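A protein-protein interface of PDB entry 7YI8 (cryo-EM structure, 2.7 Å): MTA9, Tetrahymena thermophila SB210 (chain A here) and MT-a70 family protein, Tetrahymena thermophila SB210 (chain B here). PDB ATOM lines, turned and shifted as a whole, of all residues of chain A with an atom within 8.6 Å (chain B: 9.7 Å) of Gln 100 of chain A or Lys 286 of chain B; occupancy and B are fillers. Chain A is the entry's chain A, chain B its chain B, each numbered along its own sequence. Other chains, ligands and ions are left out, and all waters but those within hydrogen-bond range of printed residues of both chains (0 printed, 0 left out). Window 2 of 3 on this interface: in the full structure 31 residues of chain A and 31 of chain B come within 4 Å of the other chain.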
ATOM      1  N   ASP A  98      11.704 -18.368 -12.147  1.00  0.00           N
ATOM      2  CA  ASP A  98      12.769 -17.838 -12.991  1.00  0.00           C
ATOM      3  C   ASP A  98      13.625 -18.962 -13.563  1.00  0.00           C
ATOM      4  O   ASP A  98      13.488 -19.326 -14.731  1.00  0.00           O
ATOM      5  CB  ASP A  98      13.641 -16.859 -12.202  1.00  0.00           C
ATOM      6  CG  ASP A  98      12.987 -15.502 -12.033  1.00  0.00           C
ATOM      7  OD1 ASP A  98      11.746 -15.452 -11.905  1.00  0.00           O
ATOM      8  OD2 ASP A  98      13.714 -14.487 -12.030  1.00  0.00           O
ATOM      9  N   ASN A  99      14.515 -19.504 -12.729  1.00  0.00           N
ATOM     10  CA  ASN A  99      15.363 -20.610 -13.162  1.00  0.00           C
ATOM     11  C   ASN A  99      14.545 -21.859 -13.456  1.00  0.00           C
ATOM     12  O   ASN A  99      14.864 -22.611 -14.384  1.00  0.00           O
ATOM     13  CB  ASN A  99      16.420 -20.912 -12.102  1.00  0.00           C
ATOM     14  CG  ASN A  99      17.746 -20.268 -12.408  1.00  0.00           C
ATOM     15  OD1 ASN A  99      18.001 -19.863 -13.539  1.00  0.00           O
ATOM     16  ND2 ASN A  99      18.606 -20.172 -11.401  1.00  0.00           N
ATOM     17  N   GLN A 100      13.494 -22.099 -12.669  1.00  0.00           N
ATOM     18  CA  GLN A 100      12.728 -23.345 -12.707  1.00  0.00           C
ATOM     19  C   GLN A 100      13.604 -24.549 -12.374  1.00  0.00           C
ATOM     20  O   GLN A 100      13.305 -25.677 -12.772  1.00  0.00           O
ATOM     21  CB  GLN A 100      12.030 -23.546 -14.058  1.00  0.00           C
ATOM     22  CG  GLN A 100      11.401 -22.290 -14.633  1.00  0.00           C
ATOM     23  CD  GLN A 100      10.008 -22.041 -14.100  1.00  0.00           C
ATOM     24  OE1 GLN A 100       9.205 -22.965 -13.974  1.00  0.00           O
ATOM     25  NE2 GLN A 100       9.712 -20.787 -13.780  1.00  0.00           N
ATOM     26  N   LEU A 101      14.692 -24.315 -11.632  1.00  0.00           N
ATOM     27  CA  LEU A 101      15.563 -25.403 -11.205  1.00  0.00           C
ATOM     28  C   LEU A 101      14.866 -26.356 -10.243  1.00  0.00           C
ATOM     29  O   LEU A 101      15.284 -27.510 -10.126  1.00  0.00           O
ATOM     30  CB  LEU A 101      16.828 -24.846 -10.553  1.00  0.00           C
ATOM     31  CG  LEU A 101      18.002 -24.536 -11.484  1.00  0.00           C
ATOM     32  CD1 LEU A 101      19.280 -24.351 -10.686  1.00  0.00           C
ATOM     33  CD2 LEU A 101      18.174 -25.628 -12.523  1.00  0.00           C
ATOM     34  N   SER A 102      13.822 -25.897  -9.551  1.00  0.00           N
ATOM     35  CA  SER A 102      13.018 -26.801  -8.739  1.00  0.00           C
ATOM     36  C   SER A 102      12.289 -27.831  -9.588  1.00  0.00           C
ATOM     37  O   SER A 102      11.898 -28.881  -9.069  1.00  0.00           O
ATOM     38  CB  SER A 102      12.011 -26.007  -7.906  1.00  0.00           C
ATOM     39  OG  SER A 102      12.661 -24.996  -7.156  1.00  0.00           O
ATOM     40  N   LEU A 103      12.096 -27.550 -10.875  1.00  0.00           N
ATOM     41  CA  LEU A 103      11.505 -28.500 -11.806  1.00  0.00           C
ATOM     42  C   LEU A 103      12.540 -29.205 -12.669  1.00  0.00           C
ATOM     43  O   LEU A 103      12.323 -30.356 -13.062  1.00  0.00           O
ATOM     44  CB  LEU A 103      10.490 -27.788 -12.708  1.00  0.00           C
ATOM     45  CG  LEU A 103       9.719 -28.645 -13.711  1.00  0.00           C
ATOM     46  CD1 LEU A 103       8.863 -29.671 -12.987  1.00  0.00           C
ATOM     47  CD2 LEU A 103       8.860 -27.772 -14.610  1.00  0.00           C
ATOM     48  N   LEU A 104      13.661 -28.545 -12.967  1.00  0.00           N
ATOM     49  CA  LEU A 104      14.711 -29.185 -13.751  1.00  0.00           C
ATOM     50  C   LEU A 104      15.389 -30.299 -12.963  1.00  0.00           C
ATOM     51  O   LEU A 104      15.746 -31.340 -13.528  1.00  0.00           O
ATOM     52  CB  LEU A 104      15.737 -28.147 -14.200  1.00  0.00           C
ATOM     53  CG  LEU A 104      15.302 -27.164 -15.289  1.00  0.00           C
ATOM     54  CD1 LEU A 104      16.509 -26.444 -15.870  1.00  0.00           C
ATOM     55  CD2 LEU A 104      14.518 -27.872 -16.381  1.00  0.00           C
ATOM     56  N   LEU A 105      15.578 -30.099 -11.658  1.00  0.00           N
ATOM     57  CA  LEU A 105      16.227 -31.074 -10.791  1.00  0.00           C
ATOM     58  C   LEU A 105      15.244 -31.738  -9.833  1.00  0.00           C
ATOM     59  O   LEU A 105      15.649 -32.229  -8.777  1.00  0.00           O
ATOM     60  CB  LEU A 105      17.361 -30.410 -10.012  1.00  0.00           C
ATOM     61  CG  LEU A 105      18.484 -29.824 -10.867  1.00  0.00           C
ATOM     62  CD1 LEU A 105      19.481 -29.057 -10.015  1.00  0.00           C
ATOM     63  CD2 LEU A 105      19.180 -30.925 -11.646  1.00  0.00           C
ATOM     64  N   LYS A 106      13.957 -31.758 -10.184  1.00  0.00           N
ATOM     65  CA  LYS A 106      12.955 -32.340  -9.296  1.00  0.00           C
ATOM     66  C   LYS A 106      13.180 -33.836  -9.110  1.00  0.00           C
ATOM     67  O   LYS A 106      12.976 -34.370  -8.014  1.00  0.00           O
ATOM     68  CB  LYS A 106      11.555 -32.070  -9.843  1.00  0.00           C
ATOM     69  CG  LYS A 106      10.439 -32.744  -9.065  1.00  0.00           C
ATOM     70  CD  LYS A 106       9.107 -32.598  -9.778  1.00  0.00           C
ATOM     71  CE  LYS A 106       9.228 -32.947 -11.252  1.00  0.00           C
ATOM     72  NZ  LYS A 106       9.624 -34.366 -11.460  1.00  0.00           N
ATOM     73  N   LEU A 335      17.257 -24.981  -2.705  1.00  0.00           N
ATOM     74  CA  LEU A 335      16.887 -24.818  -4.105  1.00  0.00           C
ATOM     75  C   LEU A 335      16.115 -23.531  -4.368  1.00  0.00           C
ATOM     76  O   LEU A 335      15.981 -23.133  -5.529  1.00  0.00           O
ATOM     77  CB  LEU A 335      16.059 -26.017  -4.580  1.00  0.00           C
ATOM     78  CG  LEU A 335      14.609 -26.165  -4.109  1.00  0.00           C
ATOM     79  CD1 LEU A 335      13.882 -27.176  -4.980  1.00  0.00           C
ATOM     80  CD2 LEU A 335      14.521 -26.577  -2.646  1.00  0.00           C
ATOM     81  N   LEU A 338      18.975 -19.840  -5.033  1.00  0.00           N
ATOM     82  CA  LEU A 338      19.640 -19.499  -6.281  1.00  0.00           C
ATOM     83  C   LEU A 338      18.686 -19.468  -7.468  1.00  0.00           C
ATOM     84  O   LEU A 338      19.143 -19.396  -8.613  1.00  0.00           O
ATOM     85  CB  LEU A 338      20.792 -20.475  -6.559  1.00  0.00           C
ATOM     86  CG  LEU A 338      20.504 -21.915  -6.998  1.00  0.00           C
ATOM     87  CD1 LEU A 338      21.764 -22.542  -7.561  1.00  0.00           C
ATOM     88  CD2 LEU A 338      19.965 -22.763  -5.861  1.00  0.00           C
ATOM     89  N   LYS A 339      17.373 -19.513  -7.220  1.00  0.00           N
ATOM     90  CA  LYS A 339      16.398 -19.454  -8.304  1.00  0.00           C
ATOM     91  C   LYS A 339      16.415 -18.116  -9.033  1.00  0.00           C
ATOM     92  O   LYS A 339      15.861 -18.018 -10.132  1.00  0.00           O
ATOM     93  CB  LYS A 339      14.994 -19.729  -7.764  1.00  0.00           C
ATOM     94  CG  LYS A 339      14.219 -18.479  -7.381  1.00  0.00           C
ATOM     95  CD  LYS A 339      12.793 -18.812  -6.984  1.00  0.00           C
ATOM     96  CE  LYS A 339      12.709 -19.201  -5.519  1.00  0.00           C
ATOM     97  NZ  LYS A 339      11.302 -19.267  -5.040  1.00  0.00           N
ATOM     98  N   SER A 340      17.031 -17.089  -8.450  1.00  0.00           N
ATOM     99  CA  SER A 340      17.155 -15.793  -9.100  1.00  0.00           C
ATOM    100  C   SER A 340      18.345 -15.718 -10.046  1.00  0.00           C
ATOM    101  O   SER A 340      18.531 -14.688 -10.703  1.00  0.00           O
ATOM    102  CB  SER A 340      17.263 -14.687  -8.048  1.00  0.00           C
ATOM    103  OG  SER A 340      18.326 -14.945  -7.149  1.00  0.00           O
ATOM    104  N   THR A 341      19.150 -16.774 -10.130  1.00  0.00           N
ATOM    105  CA  THR A 341      20.315 -16.795 -10.997  1.00  0.00           C
ATOM    106  C   THR A 341      19.875 -17.147 -12.420  1.00  0.00           C
ATOM    107  O   THR A 341      18.695 -17.383 -12.690  1.00  0.00           O
ATOM    108  CB  THR A 341      21.347 -17.782 -10.445  1.00  0.00           C
ATOM    109  OG1 THR A 341      21.443 -17.610  -9.027  1.00  0.00           O
ATOM    110  CG2 THR A 341      22.734 -17.523 -11.033  1.00  0.00           C
ATOM    111  N   ILE A 343      20.477 -19.818 -15.621  1.00  0.00           N
ATOM    112  CA  ILE A 343      20.960 -21.180 -15.842  1.00  0.00           C
ATOM    113  C   ILE A 343      22.253 -21.180 -16.645  1.00  0.00           C
ATOM    114  O   ILE A 343      23.127 -22.029 -16.432  1.00  0.00           O
ATOM    115  CB  ILE A 343      19.870 -22.025 -16.532  1.00  0.00           C
ATOM    116  CG1 ILE A 343      18.642 -22.150 -15.636  1.00  0.00           C
ATOM    117  CG2 ILE A 343      20.389 -23.410 -16.870  1.00  0.00           C
ATOM    118  CD1 ILE A 343      17.444 -22.738 -16.335  1.00  0.00           C
ATOM    119  N   PHE A 387      18.678 -33.231 -16.791  1.00  0.00           N
ATOM    120  CA  PHE A 387      19.543 -32.253 -16.144  1.00  0.00           C
ATOM    121  C   PHE A 387      20.129 -32.848 -14.871  1.00  0.00           C
ATOM    122  O   PHE A 387      19.419 -33.493 -14.095  1.00  0.00           O
ATOM    123  CB  PHE A 387      18.772 -30.970 -15.817  1.00  0.00           C
ATOM    124  CG  PHE A 387      18.738 -29.977 -16.944  1.00  0.00           C
ATOM    125  CD1 PHE A 387      19.752 -29.047 -17.095  1.00  0.00           C
ATOM    126  CD2 PHE A 387      17.693 -29.973 -17.848  1.00  0.00           C
ATOM    127  CE1 PHE A 387      19.722 -28.133 -18.129  1.00  0.00           C
ATOM    128  CE2 PHE A 387      17.659 -29.062 -18.883  1.00  0.00           C
ATOM    129  CZ  PHE A 387      18.674 -28.142 -19.024  1.00  0.00           C
ATOM    130  N   VAL B 279      18.736 -27.051 -27.089  1.00  0.00           N
ATOM    131  CA  VAL B 279      17.629 -27.450 -26.231  1.00  0.00           C
ATOM    132  C   VAL B 279      16.575 -26.353 -26.262  1.00  0.00           C
ATOM    133  O   VAL B 279      16.890 -25.153 -26.175  1.00  0.00           O
ATOM    134  CB  VAL B 279      18.111 -27.723 -24.792  1.00  0.00           C
ATOM    135  CG1 VAL B 279      16.945 -28.104 -23.897  1.00  0.00           C
ATOM    136  CG2 VAL B 279      19.178 -28.804 -24.783  1.00  0.00           C
ATOM    137  N   LYS B 280      15.319 -26.767 -26.402  1.00  0.00           N
ATOM    138  CA  LYS B 280      14.210 -25.857 -26.643  1.00  0.00           C
ATOM    139  C   LYS B 280      13.538 -25.480 -25.329  1.00  0.00           C
ATOM    140  O   LYS B 280      13.217 -26.348 -24.511  1.00  0.00           O
ATOM    141  CB  LYS B 280      13.203 -26.500 -27.595  1.00  0.00           C
ATOM    142  CG  LYS B 280      13.758 -26.746 -28.987  1.00  0.00           C
ATOM    143  CD  LYS B 280      12.725 -27.391 -29.891  1.00  0.00           C
ATOM    144  CE  LYS B 280      13.263 -27.548 -31.302  1.00  0.00           C
ATOM    145  NZ  LYS B 280      14.385 -28.522 -31.358  1.00  0.00           N
ATOM    146  N   LYS B 281      13.320 -24.183 -25.144  1.00  0.00           N
ATOM    147  CA  LYS B 281      12.802 -23.612 -23.914  1.00  0.00           C
ATOM    148  C   LYS B 281      11.440 -22.987 -24.168  1.00  0.00           C
ATOM    149  O   LYS B 281      11.175 -22.460 -25.251  1.00  0.00           O
ATOM    150  CB  LYS B 281      13.765 -22.551 -23.364  1.00  0.00           C
ATOM    151  CG  LYS B 281      13.911 -22.535 -21.862  1.00  0.00           C
ATOM    152  CD  LYS B 281      14.462 -21.204 -21.386  1.00  0.00           C
ATOM    153  CE  LYS B 281      15.761 -20.864 -22.082  1.00  0.00           C
ATOM    154  NZ  LYS B 281      16.498 -19.790 -21.368  1.00  0.00           N
ATOM    155  N   THR B 282      10.575 -23.048 -23.160  1.00  0.00           N
ATOM    156  CA  THR B 282       9.262 -22.431 -23.261  1.00  0.00           C
ATOM    157  C   THR B 282       9.345 -20.956 -22.868  1.00  0.00           C
ATOM    158  O   THR B 282      10.423 -20.410 -22.615  1.00  0.00           O
ATOM    159  CB  THR B 282       8.251 -23.173 -22.388  1.00  0.00           C
ATOM    160  OG1 THR B 282       8.696 -23.170 -21.026  1.00  0.00           O
ATOM    161  CG2 THR B 282       8.092 -24.608 -22.859  1.00  0.00           C
ATOM    162  N   VAL B 283       8.184 -20.301 -22.824  1.00  0.00           N
ATOM    163  CA  VAL B 283       8.134 -18.903 -22.409  1.00  0.00           C
ATOM    164  C   VAL B 283       8.512 -18.767 -20.939  1.00  0.00           C
ATOM    165  O   VAL B 283       9.144 -17.783 -20.534  1.00  0.00           O
ATOM    166  CB  VAL B 283       6.744 -18.308 -22.701  1.00  0.00           C
ATOM    167  CG1 VAL B 283       6.513 -18.215 -24.199  1.00  0.00           C
ATOM    168  CG2 VAL B 283       5.655 -19.148 -22.052  1.00  0.00           C
ATOM    169  N   ASN B 284       8.133 -19.748 -20.117  1.00  0.00           N
ATOM    170  CA  ASN B 284       8.439 -19.683 -18.693  1.00  0.00           C
ATOM    171  C   ASN B 284       9.912 -19.965 -18.427  1.00  0.00           C
ATOM    172  O   ASN B 284      10.535 -19.304 -17.587  1.00  0.00           O
ATOM    173  CB  ASN B 284       7.559 -20.670 -17.928  1.00  0.00           C
ATOM    174  CG  ASN B 284       6.104 -20.592 -18.341  1.00  0.00           C
ATOM    175  OD1 ASN B 284       5.533 -19.506 -18.443  1.00  0.00           O
ATOM    176  ND2 ASN B 284       5.497 -21.746 -18.588  1.00  0.00           N
ATOM    177  N   GLY B 285      10.485 -20.939 -19.129  1.00  0.00           N
ATOM    178  CA  GLY B 285      11.862 -21.332 -18.901  1.00  0.00           C
ATOM    179  C   GLY B 285      12.022 -22.831 -18.753  1.00  0.00           C
ATOM    180  O   GLY B 285      13.088 -23.316 -18.368  1.00  0.00           O
ATOM    181  N   LYS B 286      10.959 -23.572 -19.059  1.00  0.00           N
ATOM    182  CA  LYS B 286      10.939 -25.020 -18.922  1.00  0.00           C
ATOM    183  C   LYS B 286      11.486 -25.670 -20.193  1.00  0.00           C
ATOM    184  O   LYS B 286      12.063 -25.010 -21.059  1.00  0.00           O
ATOM    185  CB  LYS B 286       9.523 -25.495 -18.607  1.00  0.00           C
ATOM    186  CG  LYS B 286       8.872 -24.770 -17.444  1.00  0.00           C
ATOM    187  CD  LYS B 286       7.540 -25.402 -17.081  1.00  0.00           C
ATOM    188  CE  LYS B 286       6.709 -24.473 -16.215  1.00  0.00           C
ATOM    189  NZ  LYS B 286       7.405 -24.132 -14.946  1.00  0.00           N
ATOM    190  N   ILE B 287      11.309 -26.984 -20.313  1.00  0.00           N
ATOM    191  CA  ILE B 287      11.785 -27.748 -21.461  1.00  0.00           C
ATOM    192  C   ILE B 287      10.614 -27.991 -22.402  1.00  0.00           C
ATOM    193  O   ILE B 287       9.554 -28.469 -21.978  1.00  0.00           O
ATOM    194  CB  ILE B 287      12.418 -29.079 -21.021  1.00  0.00           C
ATOM    195  CG1 ILE B 287      13.592 -28.828 -20.074  1.00  0.00           C
ATOM    196  CG2 ILE B 287      12.890 -29.869 -22.227  1.00  0.00           C
ATOM    197  CD1 ILE B 287      14.703 -28.031 -20.692  1.00  0.00           C
ATOM    198  N   ALA B 288      10.801 -27.660 -23.677  1.00  0.00           N
ATOM    199  CA  ALA B 288       9.762 -27.877 -24.675  1.00  0.00           C
ATOM    200  C   ALA B 288       9.726 -29.339 -25.097  1.00  0.00           C
ATOM    201  O   ALA B 288      10.767 -29.971 -25.293  1.00  0.00           O
ATOM    202  CB  ALA B 288       9.998 -26.985 -25.893  1.00  0.00           C
ATOM    203  N   LYS B 289       8.516 -29.873 -25.240  1.00  0.00           N
ATOM    204  CA  LYS B 289       8.306 -31.272 -25.586  1.00  0.00           C
ATOM    205  C   LYS B 289       7.815 -31.381 -27.021  1.00  0.00           C
ATOM    206  O   LYS B 289       6.853 -30.710 -27.407  1.00  0.00           O
ATOM    207  CB  LYS B 289       7.298 -31.927 -24.636  1.00  0.00           C
ATOM    208  CG  LYS B 289       7.692 -31.935 -23.158  1.00  0.00           C
ATOM    209  CD  LYS B 289       8.842 -32.891 -22.856  1.00  0.00           C
ATOM    210  CE  LYS B 289      10.197 -32.194 -22.889  1.00  0.00           C
ATOM    211  NZ  LYS B 289      11.302 -33.101 -22.491  1.00  0.00           N
ATOM    212  N   ALA B 298      13.447 -33.390 -27.369  1.00  0.00           N
ATOM    213  CA  ALA B 298      13.488 -32.059 -26.775  1.00  0.00           C
ATOM    214  C   ALA B 298      14.760 -31.307 -27.150  1.00  0.00           C
ATOM    215  O   ALA B 298      15.137 -30.357 -26.461  1.00  0.00           O
ATOM    216  CB  ALA B 298      13.355 -32.142 -25.253  1.00  0.00           C
ATOM    217  N   PHE B 325      20.801 -23.426 -24.891  1.00  0.00           N
ATOM    218  CA  PHE B 325      19.519 -23.523 -24.192  1.00  0.00           C
ATOM    219  C   PHE B 325      18.712 -22.273 -24.524  1.00  0.00           C
ATOM    220  O   PHE B 325      18.895 -21.222 -23.904  1.00  0.00           O
ATOM    221  CB  PHE B 325      19.751 -23.681 -22.693  1.00  0.00           C
ATOM    222  CG  PHE B 325      18.515 -24.027 -21.915  1.00  0.00           C
ATOM    223  CD1 PHE B 325      17.593 -24.924 -22.418  1.00  0.00           C
ATOM    224  CD2 PHE B 325      18.297 -23.483 -20.663  1.00  0.00           C
ATOM    225  CE1 PHE B 325      16.463 -25.249 -21.698  1.00  0.00           C
ATOM    226  CE2 PHE B 325      17.169 -23.810 -19.937  1.00  0.00           C
ATOM    227  CZ  PHE B 325      16.254 -24.695 -20.454  1.00  0.00           C
ATOM    228  N   SER B 326      17.811 -22.378 -25.504  1.00  0.00           N
ATOM    229  CA  SER B 326      17.155 -21.189 -26.038  1.00  0.00           C
ATOM    230  C   SER B 326      15.706 -21.488 -26.386  1.00  0.00           C
ATOM    231  O   SER B 326      15.296 -22.642 -26.511  1.00  0.00           O
ATOM    232  CB  SER B 326      17.888 -20.646 -27.267  1.00  0.00           C
ATOM    233  OG  SER B 326      18.997 -19.857 -26.882  1.00  0.00           O
ATOM    234  N   GLU B 327      14.928 -20.418 -26.541  1.00  0.00           N
ATOM    235  CA  GLU B 327      13.495 -20.529 -26.772  1.00  0.00           C
ATOM    236  C   GLU B 327      13.192 -20.901 -28.219  1.00  0.00           C
ATOM    237  O   GLU B 327      13.929 -20.548 -29.146  1.00  0.00           O
ATOM    238  CB  GLU B 327      12.792 -19.218 -26.419  1.00  0.00           C
ATOM    239  CG  GLU B 327      12.823 -18.880 -24.939  1.00  0.00           C
ATOM    240  CD  GLU B 327      12.136 -17.565 -24.623  1.00  0.00           C
ATOM    241  OE1 GLU B 327      11.744 -16.853 -25.572  1.00  0.00           O
ATOM    242  OE2 GLU B 327      11.990 -17.242 -23.425  1.00  0.00           O
ATOM    243  N   ARG B 328      12.083 -21.611 -28.404  1.00  0.00           N
ATOM    244  CA  ARG B 328      11.672 -22.089 -29.719  1.00  0.00           C
ATOM    245  C   ARG B 328      10.921 -20.981 -30.449  1.00  0.00           C
ATOM    246  O   ARG B 328       9.803 -20.620 -30.067  1.00  0.00           O
ATOM    247  CB  ARG B 328      10.808 -23.339 -29.578  1.00  0.00           C
ATOM    248  CG  ARG B 328      10.456 -24.006 -30.893  1.00  0.00           C
ATOM    249  CD  ARG B 328       9.453 -25.125 -30.683  1.00  0.00           C
ATOM    250  NE  ARG B 328       8.354 -24.715 -29.818  1.00  0.00           N
ATOM    251  CZ  ARG B 328       7.609 -25.549 -29.104  1.00  0.00           C
ATOM    252  NH1 ARG B 328       7.819 -26.854 -29.125  1.00  0.00           N
ATOM    253  NH2 ARG B 328       6.629 -25.059 -28.350  1.00  0.00           N
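N of Ile 343 of chain A lies close to OD1 of Asn 99 of chain A.
The backbone NH of Lys 286 of chain B lies within hydrogen-bond range of the side-chain hydroxyl of Thr 282 of chain B, 3.0 Å away.
Gln 100 of chain A touches one residue of chain B.
Of the printed residues of chain A, Lys 286 of chain B touches Gln 100 (2.4 Å) and Leu 103 (3.7 Å).
Ser 102 of chain A touches none of the printed residues of chain B.
No residue of chain A comes within 4 Å of Gly 285 of chain B.
Printed residues of chain B within 4 Å of Ile 343 of chain A: Phe 325.
Printed residues of chain A within 4 Å of Phe 325 of chain B: Ile 343 (3.8 Å).
Of the printed residues of chain B, Leu 103 of chain A touches Lys 286.
Of the printed residues of chain B, Phe 387 of chain A touches Ile 287 (3.6 Å).
Thr 341 of chain A touches none of the printed residues of chain B.
Ala 288 of chain B touches none of the printed residues of chain A.
The side-chain amide oxygen (OE1) of Gln 100 of chain A lies close to the side-chain amino group (NZ) of Lys 286 of chain B, 2.4 Å away.
CD of Lys 286 of chain B touches CD2 of Leu 103 of chain A, 3.7 Å away.
Leu 104 of chain A touches Ile 287 of chain B (CD2 to CG1, 3.9 Å).
Ile 343 of chain A touches Phe 325 of chain B.
CE2 of Phe 387 of chain A touches CD1 of Ile 287 of chain B (3.6 Å).
Of the 16 printed residues of chain B, 3 touch a printed residue of chain A.
Among the printed residues, no Asp or Glu carboxylate lies within 4 Å of a Lys or Arg side-chain nitrogen of the other chain.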
